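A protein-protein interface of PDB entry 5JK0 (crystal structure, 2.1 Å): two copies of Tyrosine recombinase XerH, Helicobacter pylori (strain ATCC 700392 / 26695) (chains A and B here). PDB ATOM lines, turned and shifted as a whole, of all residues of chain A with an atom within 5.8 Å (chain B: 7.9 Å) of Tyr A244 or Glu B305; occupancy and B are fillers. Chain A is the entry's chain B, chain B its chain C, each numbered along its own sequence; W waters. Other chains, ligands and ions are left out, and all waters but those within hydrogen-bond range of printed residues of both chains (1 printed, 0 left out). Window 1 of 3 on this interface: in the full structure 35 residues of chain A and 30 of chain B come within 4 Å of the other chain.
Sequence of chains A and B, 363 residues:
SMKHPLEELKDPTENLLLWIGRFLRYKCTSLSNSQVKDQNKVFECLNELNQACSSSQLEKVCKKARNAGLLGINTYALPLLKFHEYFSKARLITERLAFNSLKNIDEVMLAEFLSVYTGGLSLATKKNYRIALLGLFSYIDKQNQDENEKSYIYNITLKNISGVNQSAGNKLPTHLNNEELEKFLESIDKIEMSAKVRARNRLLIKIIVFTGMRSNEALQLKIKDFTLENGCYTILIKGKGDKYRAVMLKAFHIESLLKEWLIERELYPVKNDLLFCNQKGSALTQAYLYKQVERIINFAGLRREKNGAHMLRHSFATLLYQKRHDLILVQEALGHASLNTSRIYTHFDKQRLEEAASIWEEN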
ATOM      1  N   LYS A 222      13.630 -29.701  -8.705  1.00  0.00           N
ATOM      2  CA  LYS A 222      12.915 -28.533  -9.204  1.00  0.00           C
ATOM      3  C   LYS A 222      13.840 -27.660 -10.041  1.00  0.00           C
ATOM      4  O   LYS A 222      15.061 -27.733  -9.907  1.00  0.00           O
ATOM      5  CB  LYS A 222      12.332 -27.716  -8.050  1.00  0.00           C
ATOM      6  CG  LYS A 222      11.274 -28.437  -7.236  1.00  0.00           C
ATOM      7  CD  LYS A 222      10.725 -27.530  -6.145  1.00  0.00           C
ATOM      8  CE  LYS A 222       9.660 -28.231  -5.323  1.00  0.00           C
ATOM      9  NZ  LYS A 222       9.133 -27.350  -4.247  1.00  0.00           N
ATOM     10  N   LYS A 224      14.216 -24.472  -9.790  1.00  0.00           N
ATOM     11  CA  LYS A 224      14.847 -23.473  -8.935  1.00  0.00           C
ATOM     12  C   LYS A 224      15.921 -24.071  -8.027  1.00  0.00           C
ATOM     13  O   LYS A 224      16.517 -23.366  -7.212  1.00  0.00           O
ATOM     14  CB  LYS A 224      13.794 -22.749  -8.095  1.00  0.00           C
ATOM     15  CG  LYS A 224      13.147 -23.591  -7.012  1.00  0.00           C
ATOM     16  CD  LYS A 224      12.174 -22.744  -6.201  1.00  0.00           C
ATOM     17  CE  LYS A 224      11.630 -23.496  -5.001  1.00  0.00           C
ATOM     18  NZ  LYS A 224      10.726 -22.637  -4.182  1.00  0.00           N
ATOM     19  N   ASP A 225      16.164 -25.371  -8.168  1.00  0.00           N
ATOM     20  CA  ASP A 225      17.278 -26.015  -7.480  1.00  0.00           C
ATOM     21  C   ASP A 225      18.578 -25.764  -8.242  1.00  0.00           C
ATOM     22  O   ASP A 225      19.668 -26.070  -7.752  1.00  0.00           O
ATOM     23  CB  ASP A 225      17.034 -27.519  -7.332  1.00  0.00           C
ATOM     24  CG  ASP A 225      15.856 -27.837  -6.427  1.00  0.00           C
ATOM     25  OD1 ASP A 225      15.544 -27.017  -5.538  1.00  0.00           O
ATOM     26  OD2 ASP A 225      15.241 -28.908  -6.606  1.00  0.00           O
ATOM     27  N   THR A 227      21.259 -23.190 -10.107  1.00  0.00           N
ATOM     28  CA  THR A 227      21.801 -21.847 -10.291  1.00  0.00           C
ATOM     29  C   THR A 227      23.090 -21.915 -11.105  1.00  0.00           C
ATOM     30  O   THR A 227      23.939 -22.776 -10.871  1.00  0.00           O
ATOM     31  CB  THR A 227      22.084 -21.136  -8.949  1.00  0.00           C
ATOM     32  OG1 THR A 227      23.016 -21.906  -8.179  1.00  0.00           O
ATOM     33  CG2 THR A 227      20.800 -20.947  -8.154  1.00  0.00           C
ATOM     34  N   LEU A 236      21.025 -27.865  -5.722  1.00  0.00           N
ATOM     35  CA  LEU A 236      20.656 -28.071  -4.328  1.00  0.00           C
ATOM     36  C   LEU A 236      19.757 -29.293  -4.180  1.00  0.00           C
ATOM     37  O   LEU A 236      18.696 -29.370  -4.798  1.00  0.00           O
ATOM     38  CB  LEU A 236      19.963 -26.828  -3.769  1.00  0.00           C
ATOM     39  CG  LEU A 236      20.831 -25.572  -3.692  1.00  0.00           C
ATOM     40  CD1 LEU A 236      20.049 -24.407  -3.114  1.00  0.00           C
ATOM     41  CD2 LEU A 236      22.081 -25.846  -2.871  1.00  0.00           C
ATOM     42  N   ILE A 237      20.189 -30.246  -3.360  1.00  0.00           N
ATOM     43  CA  ILE A 237      19.442 -31.484  -3.160  1.00  0.00           C
ATOM     44  C   ILE A 237      18.831 -31.553  -1.763  1.00  0.00           C
ATOM     45  O   ILE A 237      19.551 -31.561  -0.764  1.00  0.00           O
ATOM     46  CB  ILE A 237      20.337 -32.719  -3.378  1.00  0.00           C
ATOM     47  CG1 ILE A 237      21.010 -32.659  -4.751  1.00  0.00           C
ATOM     48  CG2 ILE A 237      19.525 -33.997  -3.229  1.00  0.00           C
ATOM     49  CD1 ILE A 237      22.045 -33.741  -4.971  1.00  0.00           C
ATOM     50  N   LYS A 238      17.503 -31.602  -1.700  1.00  0.00           N
ATOM     51  CA  LYS A 238      16.789 -31.677  -0.428  1.00  0.00           C
ATOM     52  C   LYS A 238      16.838 -33.090   0.150  1.00  0.00           C
ATOM     53  O   LYS A 238      16.448 -34.053  -0.512  1.00  0.00           O
ATOM     54  CB  LYS A 238      15.337 -31.221  -0.603  1.00  0.00           C
ATOM     55  CG  LYS A 238      14.491 -31.261   0.663  1.00  0.00           C
ATOM     56  CD  LYS A 238      13.233 -30.413   0.504  1.00  0.00           C
ATOM     57  CE  LYS A 238      12.152 -30.812   1.497  1.00  0.00           C
ATOM     58  NZ  LYS A 238      11.659 -32.196   1.236  1.00  0.00           N
ATOM     59  N   GLY A 239      17.321 -33.208   1.384  1.00  0.00           N
ATOM     60  CA  GLY A 239      17.460 -34.504   2.024  1.00  0.00           C
ATOM     61  C   GLY A 239      16.792 -34.589   3.385  1.00  0.00           C
ATOM     62  O   GLY A 239      15.786 -33.924   3.638  1.00  0.00           O
ATOM     63  N   ASP A 242      14.814 -32.083   6.001  1.00  0.00           N
ATOM     64  CA  ASP A 242      14.472 -31.057   5.017  1.00  0.00           C
ATOM     65  C   ASP A 242      15.641 -30.106   4.761  1.00  0.00           C
ATOM     66  O   ASP A 242      15.442 -28.946   4.401  1.00  0.00           O
ATOM     67  CB  ASP A 242      13.237 -30.265   5.461  1.00  0.00           C
ATOM     68  CG  ASP A 242      11.955 -31.076   5.367  1.00  0.00           C
ATOM     69  OD1 ASP A 242      11.962 -32.129   4.695  1.00  0.00           O
ATOM     70  OD2 ASP A 242      10.939 -30.652   5.957  1.00  0.00           O
ATOM     71  N   LYS A 243      16.858 -30.609   4.949  1.00  0.00           N
ATOM     72  CA  LYS A 243      18.060 -29.813   4.734  1.00  0.00           C
ATOM     73  C   LYS A 243      18.647 -30.092   3.356  1.00  0.00           C
ATOM     74  O   LYS A 243      18.527 -31.200   2.834  1.00  0.00           O
ATOM     75  CB  LYS A 243      19.097 -30.101   5.821  1.00  0.00           C
ATOM     76  N   TYR A 244      19.284 -29.083   2.770  1.00  0.00           N
ATOM     77  CA  TYR A 244      19.841 -29.210   1.428  1.00  0.00           C
ATOM     78  C   TYR A 244      21.347 -29.456   1.438  1.00  0.00           C
ATOM     79  O   TYR A 244      22.069 -28.925   2.282  1.00  0.00           O
ATOM     80  CB  TYR A 244      19.542 -27.953   0.604  1.00  0.00           C
ATOM     81  CG  TYR A 244      18.099 -27.810   0.171  1.00  0.00           C
ATOM     82  CD1 TYR A 244      17.137 -27.309   1.039  1.00  0.00           C
ATOM     83  CD2 TYR A 244      17.703 -28.163  -1.112  1.00  0.00           C
ATOM     84  CE1 TYR A 244      15.819 -27.171   0.644  1.00  0.00           C
ATOM     85  CE2 TYR A 244      16.388 -28.028  -1.517  1.00  0.00           C
ATOM     86  CZ  TYR A 244      15.450 -27.532  -0.634  1.00  0.00           C
ATOM     87  OH  TYR A 244      14.140 -27.397  -1.033  1.00  0.00           O
ATOM     88  N   ARG A 245      21.812 -30.269   0.496  1.00  0.00           N
ATOM     89  CA  ARG A 245      23.241 -30.410   0.247  1.00  0.00           C
ATOM     90  C   ARG A 245      23.537 -29.932  -1.172  1.00  0.00           C
ATOM     91  O   ARG A 245      22.667 -29.980  -2.043  1.00  0.00           O
ATOM     92  CB  ARG A 245      23.706 -31.856   0.448  1.00  0.00           C
ATOM     93  CG  ARG A 245      23.352 -32.810  -0.686  1.00  0.00           C
ATOM     94  CD  ARG A 245      23.984 -34.175  -0.457  1.00  0.00           C
ATOM     95  NE  ARG A 245      23.779 -35.087  -1.580  1.00  0.00           N
ATOM     96  CZ  ARG A 245      22.726 -35.887  -1.709  1.00  0.00           C
ATOM     97  NH1 ARG A 245      22.622 -36.685  -2.764  1.00  0.00           N
ATOM     98  NH2 ARG A 245      21.776 -35.891  -0.784  1.00  0.00           N
ATOM     99  N   ALA A 246      24.757 -29.465  -1.403  1.00  0.00           N
ATOM    100  CA  ALA A 246      25.100 -28.872  -2.688  1.00  0.00           C
ATOM    101  C   ALA A 246      26.064 -29.737  -3.494  1.00  0.00           C
ATOM    102  O   ALA A 246      27.043 -30.260  -2.963  1.00  0.00           O
ATOM    103  CB  ALA A 246      25.691 -27.484  -2.482  1.00  0.00           C
ATOM    104  N   LYS B 171      25.301 -22.147   7.538  1.00  0.00           N
ATOM    105  CA  LYS B 171      25.305 -21.790   6.124  1.00  0.00           C
ATOM    106  C   LYS B 171      24.517 -20.507   5.873  1.00  0.00           C
ATOM    107  O   LYS B 171      23.563 -20.202   6.590  1.00  0.00           O
ATOM    108  CB  LYS B 171      24.731 -22.932   5.282  1.00  0.00           C
ATOM    109  N   PRO B 173      21.875 -17.960   4.248  1.00  0.00           N
ATOM    110  CA  PRO B 173      20.540 -18.059   3.650  1.00  0.00           C
ATOM    111  C   PRO B 173      20.598 -17.825   2.144  1.00  0.00           C
ATOM    112  O   PRO B 173      21.588 -17.281   1.652  1.00  0.00           O
ATOM    113  CB  PRO B 173      19.752 -16.943   4.350  1.00  0.00           C
ATOM    114  CG  PRO B 173      20.510 -16.668   5.609  1.00  0.00           C
ATOM    115  CD  PRO B 173      21.947 -16.895   5.262  1.00  0.00           C
ATOM    116  N   THR B 174      19.560 -18.241   1.425  1.00  0.00           N
ATOM    117  CA  THR B 174      19.493 -18.016  -0.015  1.00  0.00           C
ATOM    118  C   THR B 174      19.574 -16.522  -0.306  1.00  0.00           C
ATOM    119  O   THR B 174      18.854 -15.729   0.300  1.00  0.00           O
ATOM    120  CB  THR B 174      18.204 -18.599  -0.620  1.00  0.00           C
ATOM    121  OG1 THR B 174      18.127 -19.998  -0.320  1.00  0.00           O
ATOM    122  CG2 THR B 174      18.185 -18.408  -2.129  1.00  0.00           C
ATOM    123  N   HIS B 175      20.463 -16.142  -1.219  1.00  0.00           N
ATOM    124  CA  HIS B 175      20.715 -14.731  -1.490  1.00  0.00           C
ATOM    125  C   HIS B 175      21.386 -14.505  -2.841  1.00  0.00           C
ATOM    126  O   HIS B 175      21.790 -15.451  -3.520  1.00  0.00           O
ATOM    127  CB  HIS B 175      21.589 -14.131  -0.388  1.00  0.00           C
ATOM    128  CG  HIS B 175      23.004 -14.621  -0.409  1.00  0.00           C
ATOM    129  ND1 HIS B 175      23.376 -15.848   0.099  1.00  0.00           N
ATOM    130  CD2 HIS B 175      24.138 -14.053  -0.885  1.00  0.00           C
ATOM    131  CE1 HIS B 175      24.677 -16.012  -0.058  1.00  0.00           C
ATOM    132  NE2 HIS B 175      25.163 -14.938  -0.654  1.00  0.00           N
ATOM    133  N   TYR B 290       5.624  -9.936  -4.161  1.00  0.00           N
ATOM    134  CA  TYR B 290       6.377 -11.146  -4.467  1.00  0.00           C
ATOM    135  C   TYR B 290       6.370 -11.425  -5.967  1.00  0.00           C
ATOM    136  O   TYR B 290       7.415 -11.697  -6.558  1.00  0.00           O
ATOM    137  CB  TYR B 290       5.808 -12.352  -3.708  1.00  0.00           C
ATOM    138  CG  TYR B 290       6.554 -13.642  -3.982  1.00  0.00           C
ATOM    139  CD1 TYR B 290       6.198 -14.464  -5.046  1.00  0.00           C
ATOM    140  CD2 TYR B 290       7.619 -14.034  -3.181  1.00  0.00           C
ATOM    141  CE1 TYR B 290       6.883 -15.635  -5.307  1.00  0.00           C
ATOM    142  CE2 TYR B 290       8.309 -15.208  -3.434  1.00  0.00           C
ATOM    143  CZ  TYR B 290       7.936 -16.002  -4.500  1.00  0.00           C
ATOM    144  OH  TYR B 290       8.618 -17.169  -4.756  1.00  0.00           O
ATOM    145  N   LEU B 302      18.067 -15.480 -12.569  1.00  0.00           N
ATOM    146  CA  LEU B 302      18.601 -15.634 -11.219  1.00  0.00           C
ATOM    147  C   LEU B 302      17.698 -16.479 -10.323  1.00  0.00           C
ATOM    148  O   LEU B 302      17.812 -16.428  -9.097  1.00  0.00           O
ATOM    149  CB  LEU B 302      18.817 -14.261 -10.575  1.00  0.00           C
ATOM    150  CG  LEU B 302      19.858 -13.338 -11.212  1.00  0.00           C
ATOM    151  CD1 LEU B 302      19.851 -11.978 -10.531  1.00  0.00           C
ATOM    152  CD2 LEU B 302      21.245 -13.962 -11.144  1.00  0.00           C
ATOM    153  N   ARG B 303      16.799 -17.247 -10.933  1.00  0.00           N
ATOM    154  CA  ARG B 303      15.837 -18.048 -10.178  1.00  0.00           C
ATOM    155  C   ARG B 303      16.531 -19.052  -9.264  1.00  0.00           C
ATOM    156  O   ARG B 303      17.375 -19.831  -9.706  1.00  0.00           O
ATOM    157  CB  ARG B 303      14.880 -18.776 -11.125  1.00  0.00           C
ATOM    158  CG  ARG B 303      13.797 -19.576 -10.410  1.00  0.00           C
ATOM    159  CD  ARG B 303      12.763 -20.113 -11.386  1.00  0.00           C
ATOM    160  NE  ARG B 303      11.708 -20.861 -10.709  1.00  0.00           N
ATOM    161  CZ  ARG B 303      10.613 -20.311 -10.193  1.00  0.00           C
ATOM    162  NH1 ARG B 303      10.424 -19.000 -10.272  1.00  0.00           N
ATOM    163  NH2 ARG B 303       9.707 -21.072  -9.594  1.00  0.00           N
ATOM    164  N   ARG B 304      16.169 -19.021  -7.985  1.00  0.00           N
ATOM    165  CA  ARG B 304      16.772 -19.907  -6.999  1.00  0.00           C
ATOM    166  C   ARG B 304      15.754 -20.377  -5.959  1.00  0.00           C
ATOM    167  O   ARG B 304      14.545 -20.294  -6.180  1.00  0.00           O
ATOM    168  CB  ARG B 304      17.954 -19.207  -6.322  1.00  0.00           C
ATOM    169  CG  ARG B 304      17.694 -17.757  -5.952  1.00  0.00           C
ATOM    170  CD  ARG B 304      19.002 -16.985  -5.878  1.00  0.00           C
ATOM    171  NE  ARG B 304      19.670 -16.945  -7.177  1.00  0.00           N
ATOM    172  CZ  ARG B 304      20.957 -16.664  -7.348  1.00  0.00           C
ATOM    173  NH1 ARG B 304      21.725 -16.397  -6.301  1.00  0.00           N
ATOM    174  NH2 ARG B 304      21.478 -16.652  -8.568  1.00  0.00           N
ATOM    175  N   GLU B 305      16.249 -20.869  -4.827  1.00  0.00           N
ATOM    176  CA  GLU B 305      15.396 -21.518  -3.834  1.00  0.00           C
ATOM    177  C   GLU B 305      14.359 -20.570  -3.230  1.00  0.00           C
ATOM    178  O   GLU B 305      13.258 -20.992  -2.873  1.00  0.00           O
ATOM    179  CB  GLU B 305      16.250 -22.130  -2.724  1.00  0.00           C
ATOM    180  CG  GLU B 305      15.630 -23.368  -2.098  1.00  0.00           C
ATOM    181  CD  GLU B 305      15.373 -24.463  -3.117  1.00  0.00           C
ATOM    182  OE1 GLU B 305      16.295 -24.783  -3.898  1.00  0.00           O
ATOM    183  OE2 GLU B 305      14.245 -25.000  -3.143  1.00  0.00           O
ATOM    184  N   LYS B 306      14.716 -19.296  -3.114  1.00  0.00           N
ATOM    185  CA  LYS B 306      13.779 -18.271  -2.663  1.00  0.00           C
ATOM    186  C   LYS B 306      13.792 -17.106  -3.647  1.00  0.00           C
ATOM    187  O   LYS B 306      14.858 -16.617  -4.019  1.00  0.00           O
ATOM    188  CB  LYS B 306      14.129 -17.783  -1.255  1.00  0.00           C
ATOM    189  CG  LYS B 306      14.130 -18.867  -0.191  1.00  0.00           C
ATOM    190  CD  LYS B 306      12.741 -19.451   0.019  1.00  0.00           C
ATOM    191  CE  LYS B 306      12.757 -20.514   1.106  1.00  0.00           C
ATOM    192  NZ  LYS B 306      11.422 -21.137   1.295  1.00  0.00           N
ATOM    193  N   ASN B 307      12.613 -16.663  -4.071  1.00  0.00           N
ATOM    194  CA  ASN B 307      12.531 -15.639  -5.107  1.00  0.00           C
ATOM    195  C   ASN B 307      11.672 -14.434  -4.727  1.00  0.00           C
ATOM    196  O   ASN B 307      10.984 -13.862  -5.574  1.00  0.00           O
ATOM    197  CB  ASN B 307      12.004 -16.257  -6.403  1.00  0.00           C
ATOM    198  CG  ASN B 307      12.851 -17.426  -6.878  1.00  0.00           C
ATOM    199  OD1 ASN B 307      13.968 -17.242  -7.364  1.00  0.00           O
ATOM    200  ND2 ASN B 307      12.322 -18.635  -6.739  1.00  0.00           N
ATOM    201  N   GLY B 308      11.721 -14.041  -3.457  1.00  0.00           N
ATOM    202  CA  GLY B 308      10.925 -12.926  -2.975  1.00  0.00           C
ATOM    203  C   GLY B 308      11.732 -11.787  -2.381  1.00  0.00           C
ATOM    204  O   GLY B 308      12.962 -11.768  -2.462  1.00  0.00           O
ATOM    205  N   MET B 311      14.363 -12.561   0.335  1.00  0.00           N
ATOM    206  CA  MET B 311      15.636 -13.022  -0.208  1.00  0.00           C
ATOM    207  C   MET B 311      16.528 -11.825  -0.526  1.00  0.00           C
ATOM    208  O   MET B 311      17.749 -11.889  -0.374  1.00  0.00           O
ATOM    209  CB  MET B 311      15.409 -13.877  -1.460  1.00  0.00           C
ATOM    210  CG  MET B 311      16.660 -14.573  -1.989  1.00  0.00           C
ATOM    211  SD  MET B 311      17.632 -13.571  -3.133  1.00  0.00           S
ATOM    212  CE  MET B 311      16.522 -13.473  -4.534  1.00  0.00           C
HETATM  213  O   HOH W   1      13.523 -27.682  -3.982  1.00  0.00           O
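Among the printed residues, merely in contact across the chains: Lys A224 with Arg B304 (3.2 Å), Thr A227 with Arg B304 (3.8 Å), Lys A224 with Arg B303 (3.8 Å), Leu A236 with Glu B305 (3.9 Å) and Thr A227 with Arg B303 (3.9 Å).
Of the 13 printed residues of chain A, 5 touch a printed residue of chain B. Printed residues of chain A that touch a printed residue of chain B: Lys A224, Asp A225, Thr A227, Leu A236 and Tyr A244. Hydrophobic or aromatic side chains of chain A that line the printed part of chain B: Leu A236 and Tyr A244. Among the printed residues, 8 pairs touch across the chains.
Water W1 lies within hydrogen-bond range of the side-chain carboxylate of Asp A225 (2.6 Å), the side-chain carboxylate of Glu B305 (2.9 Å) and the side-chain hydroxyl of Tyr A244 (3.0 Å).
Of the printed residues of chain B, Lys A224 touches Arg B303 (3.8 Å), Arg B304 (3.2 Å) and Glu B305 (3.3 Å). Of the printed residues of chain B, Asp A225 touches Glu B305 (2.9 Å). Printed residues of chain B within 4 Å of Thr A227: Arg B303 (3.9 Å) and Arg B304 (3.8 Å). Printed residues of chain B within 4 Å of Leu A236: Glu B305. No residue of chain B comes within 4 Å of Lys A243. Tyr A244 touches just one residue of chain B: Glu B305. Thr B174 touches none of the printed residues of chain A. Of chain A, only Lys A224, Asp A225, Leu A236 and Tyr A244 come within 4 Å of Glu B305.
No position is printed for both chains. Of the 8 pairs that touch across the chains among the printed residues, none has its exchanged pair printed and touching as well.
The backbone NH of Lys A222 is in hydrogen-bond range of the side-chain carboxylate of Asp A225 (2.8 Å). The backbone carbonyl oxygen (O) of Leu B302 is in hydrogen-bond range of the guanidinium group (NE) of Arg B304. The backbone carbonyl oxygen (O) of His B175 sits at hydrogen-bond distance from the guanidinium group (NH1) of Arg B304 (2.9 Å). N of Leu A236 lies within hydrogen-bond range of O of Asp A225, at 3.0 Å. O of Arg B304 lies within hydrogen-bond range of ND2 of Asn B307 (2.8 Å).
OH of Tyr A244 lies within hydrogen-bond range of OE2 of Glu B305. OE1 of Glu B305 sits close to OD1 of Asp A225 (2.9 Å). The backbone carbonyl oxygen (O) of Glu B305 lies within hydrogen-bond range of the side-chain amino group (NZ) of Lys A224 (3.3 Å).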
